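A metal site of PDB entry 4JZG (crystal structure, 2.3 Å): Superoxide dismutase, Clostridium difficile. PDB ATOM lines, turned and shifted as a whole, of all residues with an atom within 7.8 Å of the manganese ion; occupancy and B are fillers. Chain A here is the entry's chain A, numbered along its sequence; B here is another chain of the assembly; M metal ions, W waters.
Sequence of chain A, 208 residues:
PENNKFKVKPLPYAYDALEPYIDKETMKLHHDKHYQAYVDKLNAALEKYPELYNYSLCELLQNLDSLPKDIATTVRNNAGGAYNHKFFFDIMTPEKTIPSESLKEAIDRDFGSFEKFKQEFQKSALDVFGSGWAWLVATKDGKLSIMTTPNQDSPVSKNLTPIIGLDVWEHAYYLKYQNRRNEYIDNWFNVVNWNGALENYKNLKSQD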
ATOM      1  N   HIS A  30      10.877  31.500  -5.971  1.00  0.00           N
ATOM      2  CA  HIS A  30      12.146  30.834  -6.198  1.00  0.00           C
ATOM      3  C   HIS A  30      12.186  30.247  -7.597  1.00  0.00           C
ATOM      4  O   HIS A  30      13.179  30.401  -8.323  1.00  0.00           O
ATOM      5  CB  HIS A  30      12.340  29.730  -5.153  1.00  0.00           C
ATOM      6  CG  HIS A  30      13.774  29.394  -4.894  1.00  0.00           C
ATOM      7  ND1 HIS A  30      14.153  28.379  -4.049  1.00  0.00           N
ATOM      8  CD2 HIS A  30      14.922  29.941  -5.373  1.00  0.00           C
ATOM      9  CE1 HIS A  30      15.473  28.312  -4.006  1.00  0.00           C
ATOM     10  NE2 HIS A  30      15.957  29.242  -4.798  1.00  0.00           N
ATOM     11  N   HIS A  31      11.113  29.583  -7.985  1.00  0.00           N
ATOM     12  CA  HIS A  31      11.043  28.968  -9.310  1.00  0.00           C
ATOM     13  C   HIS A  31      10.715  29.966 -10.422  1.00  0.00           C
ATOM     14  O   HIS A  31      11.392  30.015 -11.449  1.00  0.00           O
ATOM     15  CB  HIS A  31      10.047  27.797  -9.313  1.00  0.00           C
ATOM     16  CG  HIS A  31       9.926  27.129 -10.644  1.00  0.00           C
ATOM     17  ND1 HIS A  31       9.164  27.636 -11.669  1.00  0.00           N
ATOM     18  CD2 HIS A  31      10.480  25.988 -11.127  1.00  0.00           C
ATOM     19  CE1 HIS A  31       9.258  26.848 -12.726  1.00  0.00           C
ATOM     20  NE2 HIS A  31      10.047  25.840 -12.414  1.00  0.00           N
ATOM     21  N   HIS A  34      13.506  33.796  -9.510  1.00  0.00           N
ATOM     22  CA  HIS A  34      14.931  33.531  -9.418  1.00  0.00           C
ATOM     23  C   HIS A  34      15.452  32.562 -10.492  1.00  0.00           C
ATOM     24  O   HIS A  34      16.284  32.934 -11.312  1.00  0.00           O
ATOM     25  CB  HIS A  34      15.297  33.048  -8.006  1.00  0.00           C
ATOM     26  CG  HIS A  34      15.003  34.056  -6.940  1.00  0.00           C
ATOM     27  ND1 HIS A  34      15.923  34.985  -6.516  1.00  0.00           N
ATOM     28  CD2 HIS A  34      13.872  34.293  -6.227  1.00  0.00           C
ATOM     29  CE1 HIS A  34      15.384  35.742  -5.576  1.00  0.00           C
ATOM     30  NE2 HIS A  34      14.142  35.348  -5.388  1.00  0.00           N
ATOM     31  N   TYR A  35      14.942  31.338 -10.499  1.00  0.00           N
ATOM     32  CA  TYR A  35      15.342  30.345 -11.484  1.00  0.00           C
ATOM     33  C   TYR A  35      15.154  30.901 -12.899  1.00  0.00           C
ATOM     34  O   TYR A  35      16.059  30.846 -13.722  1.00  0.00           O
ATOM     35  CB  TYR A  35      14.557  29.038 -11.264  1.00  0.00           C
ATOM     36  CG  TYR A  35      14.822  27.883 -12.233  1.00  0.00           C
ATOM     37  CD1 TYR A  35      15.982  27.802 -12.972  1.00  0.00           C
ATOM     38  CD2 TYR A  35      13.879  26.857 -12.366  1.00  0.00           C
ATOM     39  CE1 TYR A  35      16.209  26.731 -13.848  1.00  0.00           C
ATOM     40  CE2 TYR A  35      14.091  25.784 -13.222  1.00  0.00           C
ATOM     41  CZ  TYR A  35      15.254  25.727 -13.966  1.00  0.00           C
ATOM     42  OH  TYR A  35      15.427  24.667 -14.818  1.00  0.00           O
ATOM     43  N   TYR A  38      17.936  33.467 -14.030  1.00  0.00           N
ATOM     44  CA  TYR A  38      19.205  32.867 -14.438  1.00  0.00           C
ATOM     45  C   TYR A  38      19.139  32.351 -15.892  1.00  0.00           C
ATOM     46  O   TYR A  38      20.040  32.585 -16.671  1.00  0.00           O
ATOM     47  CB  TYR A  38      19.615  31.734 -13.476  1.00  0.00           C
ATOM     48  CG  TYR A  38      19.918  32.199 -12.069  1.00  0.00           C
ATOM     49  CD1 TYR A  38      20.886  33.176 -11.830  1.00  0.00           C
ATOM     50  CD2 TYR A  38      19.259  31.667 -10.980  1.00  0.00           C
ATOM     51  CE1 TYR A  38      21.187  33.605 -10.538  1.00  0.00           C
ATOM     52  CE2 TYR A  38      19.556  32.089  -9.682  1.00  0.00           C
ATOM     53  CZ  TYR A  38      20.522  33.061  -9.465  1.00  0.00           C
ATOM     54  OH  TYR A  38      20.824  33.490  -8.187  1.00  0.00           O
ATOM     55  N   GLY A  81      23.363  29.254 -11.886  1.00  0.00           N
ATOM     56  CA  GLY A  81      22.055  29.405 -11.291  1.00  0.00           C
ATOM     57  C   GLY A  81      21.054  28.471 -11.957  1.00  0.00           C
ATOM     58  O   GLY A  81      20.208  27.888 -11.298  1.00  0.00           O
ATOM     59  N   ASN A  84      22.000  24.743 -10.887  1.00  0.00           N
ATOM     60  CA  ASN A  84      21.767  24.503  -9.456  1.00  0.00           C
ATOM     61  C   ASN A  84      20.289  24.428  -9.072  1.00  0.00           C
ATOM     62  O   ASN A  84      19.886  23.584  -8.284  1.00  0.00           O
ATOM     63  CB  ASN A  84      22.489  25.571  -8.607  1.00  0.00           C
ATOM     64  CG  ASN A  84      24.001  25.482  -8.748  1.00  0.00           C
ATOM     65  OD1 ASN A  84      24.528  24.482  -9.211  1.00  0.00           O
ATOM     66  ND2 ASN A  84      24.697  26.543  -8.343  1.00  0.00           N
ATOM     67  N   HIS A  85      19.484  25.317  -9.654  1.00  0.00           N
ATOM     68  CA  HIS A  85      18.074  25.339  -9.316  1.00  0.00           C
ATOM     69  C   HIS A  85      17.303  24.181  -9.961  1.00  0.00           C
ATOM     70  O   HIS A  85      16.443  23.574  -9.305  1.00  0.00           O
ATOM     71  CB  HIS A  85      17.461  26.707  -9.665  1.00  0.00           C
ATOM     72  CG  HIS A  85      17.852  27.788  -8.694  1.00  0.00           C
ATOM     73  ND1 HIS A  85      19.006  28.525  -8.836  1.00  0.00           N
ATOM     74  CD2 HIS A  85      17.263  28.223  -7.556  1.00  0.00           C
ATOM     75  CE1 HIS A  85      19.101  29.383  -7.824  1.00  0.00           C
ATOM     76  NE2 HIS A  85      18.047  29.225  -7.046  1.00  0.00           N
ATOM     77  N   PHE A  88      18.100  21.490  -7.677  1.00  0.00           N
ATOM     78  CA  PHE A  88      17.527  21.661  -6.344  1.00  0.00           C
ATOM     79  C   PHE A  88      16.033  21.314  -6.310  1.00  0.00           C
ATOM     80  O   PHE A  88      15.559  20.643  -5.405  1.00  0.00           O
ATOM     81  CB  PHE A  88      17.744  23.104  -5.873  1.00  0.00           C
ATOM     82  CG  PHE A  88      17.223  23.396  -4.481  1.00  0.00           C
ATOM     83  CD1 PHE A  88      17.735  22.712  -3.387  1.00  0.00           C
ATOM     84  CD2 PHE A  88      16.269  24.386  -4.274  1.00  0.00           C
ATOM     85  CE1 PHE A  88      17.273  22.998  -2.103  1.00  0.00           C
ATOM     86  CE2 PHE A  88      15.812  24.678  -2.997  1.00  0.00           C
ATOM     87  CZ  PHE A  88      16.314  23.976  -1.911  1.00  0.00           C
ATOM     88  N   PHE A  89      15.286  21.768  -7.301  1.00  0.00           N
ATOM     89  CA  PHE A  89      13.873  21.438  -7.309  1.00  0.00           C
ATOM     90  C   PHE A  89      13.655  19.933  -7.549  1.00  0.00           C
ATOM     91  O   PHE A  89      12.724  19.351  -7.004  1.00  0.00           O
ATOM     92  CB  PHE A  89      13.113  22.327  -8.299  1.00  0.00           C
ATOM     93  CG  PHE A  89      13.195  23.801  -7.973  1.00  0.00           C
ATOM     94  CD1 PHE A  89      12.963  24.259  -6.668  1.00  0.00           C
ATOM     95  CD2 PHE A  89      13.506  24.729  -8.950  1.00  0.00           C
ATOM     96  CE1 PHE A  89      13.036  25.610  -6.349  1.00  0.00           C
ATOM     97  CE2 PHE A  89      13.593  26.106  -8.643  1.00  0.00           C
ATOM     98  CZ  PHE A  89      13.361  26.540  -7.346  1.00  0.00           C
ATOM     99  N   GLY A 132      25.254  30.884  -0.954  1.00  0.00           N
ATOM    100  CA  GLY A 132      25.928  29.673  -1.388  1.00  0.00           C
ATOM    101  C   GLY A 132      25.109  28.401  -1.261  1.00  0.00           C
ATOM    102  O   GLY A 132      23.901  28.443  -1.090  1.00  0.00           O
ATOM    103  N   TRP A 133      25.804  27.265  -1.340  1.00  0.00           N
ATOM    104  CA  TRP A 133      25.159  25.958  -1.407  1.00  0.00           C
ATOM    105  C   TRP A 133      25.964  24.988  -0.580  1.00  0.00           C
ATOM    106  O   TRP A 133      27.197  25.102  -0.499  1.00  0.00           O
ATOM    107  CB  TRP A 133      25.133  25.452  -2.857  1.00  0.00           C
ATOM    108  CG  TRP A 133      24.226  26.246  -3.786  1.00  0.00           C
ATOM    109  CD1 TRP A 133      24.498  27.455  -4.360  1.00  0.00           C
ATOM    110  CD2 TRP A 133      22.919  25.855  -4.257  1.00  0.00           C
ATOM    111  NE1 TRP A 133      23.444  27.847  -5.167  1.00  0.00           N
ATOM    112  CE2 TRP A 133      22.459  26.889  -5.101  1.00  0.00           C
ATOM    113  CE3 TRP A 133      22.103  24.742  -4.043  1.00  0.00           C
ATOM    114  CZ2 TRP A 133      21.210  26.838  -5.734  1.00  0.00           C
ATOM    115  CZ3 TRP A 133      20.858  24.697  -4.683  1.00  0.00           C
ATOM    116  CH2 TRP A 133      20.425  25.741  -5.517  1.00  0.00           C
ATOM    117  N   ASN A 151      27.854  31.604  -3.896  1.00  0.00           N
ATOM    118  CA  ASN A 151      27.025  32.151  -4.967  1.00  0.00           C
ATOM    119  C   ASN A 151      26.396  31.041  -5.817  1.00  0.00           C
ATOM    120  O   ASN A 151      25.748  30.167  -5.257  1.00  0.00           O
ATOM    121  CB  ASN A 151      27.851  33.161  -5.761  1.00  0.00           C
ATOM    122  CG  ASN A 151      28.426  34.238  -4.853  1.00  0.00           C
ATOM    123  OD1 ASN A 151      27.755  34.730  -3.938  1.00  0.00           O
ATOM    124  ND2 ASN A 151      29.684  34.595  -5.084  1.00  0.00           N
ATOM    125  N   GLN A 152      26.555  31.076  -7.131  1.00  0.00           N
ATOM    126  CA  GLN A 152      26.064  29.971  -7.969  1.00  0.00           C
ATOM    127  C   GLN A 152      27.165  29.053  -8.494  1.00  0.00           C
ATOM    128  O   GLN A 152      26.996  28.391  -9.523  1.00  0.00           O
ATOM    129  CB  GLN A 152      25.211  30.484  -9.136  1.00  0.00           C
ATOM    130  CG  GLN A 152      23.936  31.241  -8.727  1.00  0.00           C
ATOM    131  CD  GLN A 152      23.012  30.417  -7.818  1.00  0.00           C
ATOM    132  OE1 GLN A 152      23.165  29.190  -7.671  1.00  0.00           O
ATOM    133  NE2 GLN A 152      22.055  31.109  -7.186  1.00  0.00           N
ATOM    134  N   ASP A 167      20.221  24.859  -1.239  1.00  0.00           N
ATOM    135  CA  ASP A 167      20.314  26.299  -1.454  1.00  0.00           C
ATOM    136  C   ASP A 167      20.249  27.024  -0.099  1.00  0.00           C
ATOM    137  O   ASP A 167      19.252  26.922   0.615  1.00  0.00           O
ATOM    138  CB  ASP A 167      19.147  26.746  -2.352  1.00  0.00           C
ATOM    139  CG  ASP A 167      19.308  28.150  -2.904  1.00  0.00           C
ATOM    140  OD1 ASP A 167      20.256  28.838  -2.490  1.00  0.00           O
ATOM    141  OD2 ASP A 167      18.491  28.573  -3.768  1.00  0.00           O
ATOM    142  N   VAL A 168      21.326  27.717   0.305  1.00  0.00           N
ATOM    143  CA  VAL A 168      21.256  28.583   1.488  1.00  0.00           C
ATOM    144  C   VAL A 168      21.374  30.078   1.158  1.00  0.00           C
ATOM    145  O   VAL A 168      21.690  30.887   2.023  1.00  0.00           O
ATOM    146  CB  VAL A 168      22.252  28.182   2.624  1.00  0.00           C
ATOM    147  CG1 VAL A 168      21.888  26.804   3.203  1.00  0.00           C
ATOM    148  CG2 VAL A 168      23.674  28.185   2.132  1.00  0.00           C
ATOM    149  N   TRP A 169      21.116  30.461  -0.087  1.00  0.00           N
ATOM    150  CA  TRP A 169      20.838  31.865  -0.349  1.00  0.00           C
ATOM    151  C   TRP A 169      19.648  32.239   0.530  1.00  0.00           C
ATOM    152  O   TRP A 169      18.738  31.435   0.753  1.00  0.00           O
ATOM    153  CB  TRP A 169      20.476  32.100  -1.810  1.00  0.00           C
ATOM    154  CG  TRP A 169      21.619  32.108  -2.779  1.00  0.00           C
ATOM    155  CD1 TRP A 169      22.525  31.096  -2.991  1.00  0.00           C
ATOM    156  CD2 TRP A 169      21.942  33.147  -3.713  1.00  0.00           C
ATOM    157  NE1 TRP A 169      23.396  31.458  -4.000  1.00  0.00           N
ATOM    158  CE2 TRP A 169      23.063  32.701  -4.460  1.00  0.00           C
ATOM    159  CE3 TRP A 169      21.399  34.398  -3.999  1.00  0.00           C
ATOM    160  CZ2 TRP A 169      23.648  33.481  -5.450  1.00  0.00           C
ATOM    161  CZ3 TRP A 169      21.985  35.179  -4.988  1.00  0.00           C
ATOM    162  CH2 TRP A 169      23.090  34.707  -5.709  1.00  0.00           C
ATOM    163  N   GLU A 170      19.635  33.474   1.020  1.00  0.00           N
ATOM    164  CA  GLU A 170      18.583  33.915   1.929  1.00  0.00           C
ATOM    165  C   GLU A 170      17.219  33.922   1.254  1.00  0.00           C
ATOM    166  O   GLU A 170      16.202  33.715   1.911  1.00  0.00           O
ATOM    167  CB  GLU A 170      18.938  35.274   2.570  1.00  0.00           C
ATOM    168  CG  GLU A 170      19.984  35.147   3.675  1.00  0.00           C
ATOM    169  CD  GLU A 170      20.541  36.484   4.168  1.00  0.00           C
ATOM    170  OE1 GLU A 170      20.628  37.437   3.359  1.00  0.00           O
ATOM    171  OE2 GLU A 170      20.903  36.575   5.355  1.00  0.00           O
ATOM    172  N   HIS A 171      17.173  34.123  -0.047  1.00  0.00           N
ATOM    173  CA  HIS A 171      15.890  34.070  -0.719  1.00  0.00           C
ATOM    174  C   HIS A 171      15.230  32.689  -0.605  1.00  0.00           C
ATOM    175  O   HIS A 171      14.032  32.567  -0.797  1.00  0.00           O
ATOM    176  CB  HIS A 171      15.980  34.504  -2.181  1.00  0.00           C
ATOM    177  CG  HIS A 171      16.771  33.588  -3.065  1.00  0.00           C
ATOM    178  ND1 HIS A 171      17.854  34.010  -3.805  1.00  0.00           N
ATOM    179  CD2 HIS A 171      16.602  32.271  -3.362  1.00  0.00           C
ATOM    180  CE1 HIS A 171      18.330  32.996  -4.500  1.00  0.00           C
ATOM    181  NE2 HIS A 171      17.596  31.932  -4.248  1.00  0.00           N
ATOM    182  N   ALA A 172      15.993  31.655  -0.290  1.00  0.00           N
ATOM    183  CA  ALA A 172      15.425  30.310  -0.238  1.00  0.00           C
ATOM    184  C   ALA A 172      14.673  30.049   1.071  1.00  0.00           C
ATOM    185  O   ALA A 172      13.903  29.092   1.176  1.00  0.00           O
ATOM    186  CB  ALA A 172      16.514  29.233  -0.467  1.00  0.00           C
ATOM    187  N   TYR A 184      15.491  26.062   8.951  1.00  0.00           N
ATOM    188  CA  TYR A 184      15.341  25.750   7.530  1.00  0.00           C
ATOM    189  C   TYR A 184      16.077  24.473   7.162  1.00  0.00           C
ATOM    190  O   TYR A 184      15.524  23.568   6.535  1.00  0.00           O
ATOM    191  CB  TYR A 184      15.868  26.919   6.683  1.00  0.00           C
ATOM    192  CG  TYR A 184      16.041  26.648   5.205  1.00  0.00           C
ATOM    193  CD1 TYR A 184      14.959  26.280   4.399  1.00  0.00           C
ATOM    194  CD2 TYR A 184      17.279  26.804   4.586  1.00  0.00           C
ATOM    195  CE1 TYR A 184      15.119  26.061   3.030  1.00  0.00           C
ATOM    196  CE2 TYR A 184      17.451  26.585   3.224  1.00  0.00           C
ATOM    197  CZ  TYR A 184      16.378  26.218   2.454  1.00  0.00           C
ATOM    198  OH  TYR A 184      16.556  26.011   1.108  1.00  0.00           O
ATOM    199  N   GLU B 170      20.143  39.752   0.804  1.00  0.00           N
ATOM    200  CA  GLU B 170      18.715  39.544   0.616  1.00  0.00           C
ATOM    201  C   GLU B 170      17.945  39.729   1.919  1.00  0.00           C
ATOM    202  O   GLU B 170      16.787  40.134   1.900  1.00  0.00           O
ATOM    203  CB  GLU B 170      18.444  38.172  -0.033  1.00  0.00           C
ATOM    204  CG  GLU B 170      18.747  38.179  -1.535  1.00  0.00           C
ATOM    205  CD  GLU B 170      18.708  36.794  -2.179  1.00  0.00           C
ATOM    206  OE1 GLU B 170      19.053  35.805  -1.499  1.00  0.00           O
ATOM    207  OE2 GLU B 170      18.359  36.705  -3.372  1.00  0.00           O
HETATM  208 MN    MN M   1      18.027  29.948  -5.091  1.00  0.00          MN
HETATM  209  O   HOH W   1      20.354  30.270  -4.950  1.00  0.00           O
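O of His 30 lies within hydrogen-bond range of N of Tyr 35, at 3.0 Å.
A ring nitrogen (ND1) of His 171 lies within hydrogen-bond range of a ring nitrogen (ND1) of His 34 (3.5 Å).
The backbone carbonyl oxygen of Asp 167 is in hydrogen-bond range of the side-chain hydroxyl of Tyr 184 (2.9 Å).
The side-chain carboxylate (OE2) of Glu 170 of chain B sits at hydrogen-bond distance from a ring nitrogen (ND1) of His 171.
N of Trp 169 lies within hydrogen-bond range of OD1 of Asp 167, 3.0 Å away.
O of Gly 81 lies within hydrogen-bond range of ND1 of His 85 (2.8 Å).
Water W1 lies within hydrogen-bond range of the side-chain carboxylate of Asp 167 (2.8 Å), the side-chain amide nitrogen of Gln 152 (2.9 Å) and the indole nitrogen of Trp 169 (3.4 Å).
The manganese ion is bound by OD2 of Asp 167 (2.0 Å), NE2 of His 85 (2.1 Å), NE2 of His 171 (2.2 Å), NE2 of His 30 (2.2 Å) and water W1 (2.4 Å).
The manganese ion has five donor atoms within binding distance.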
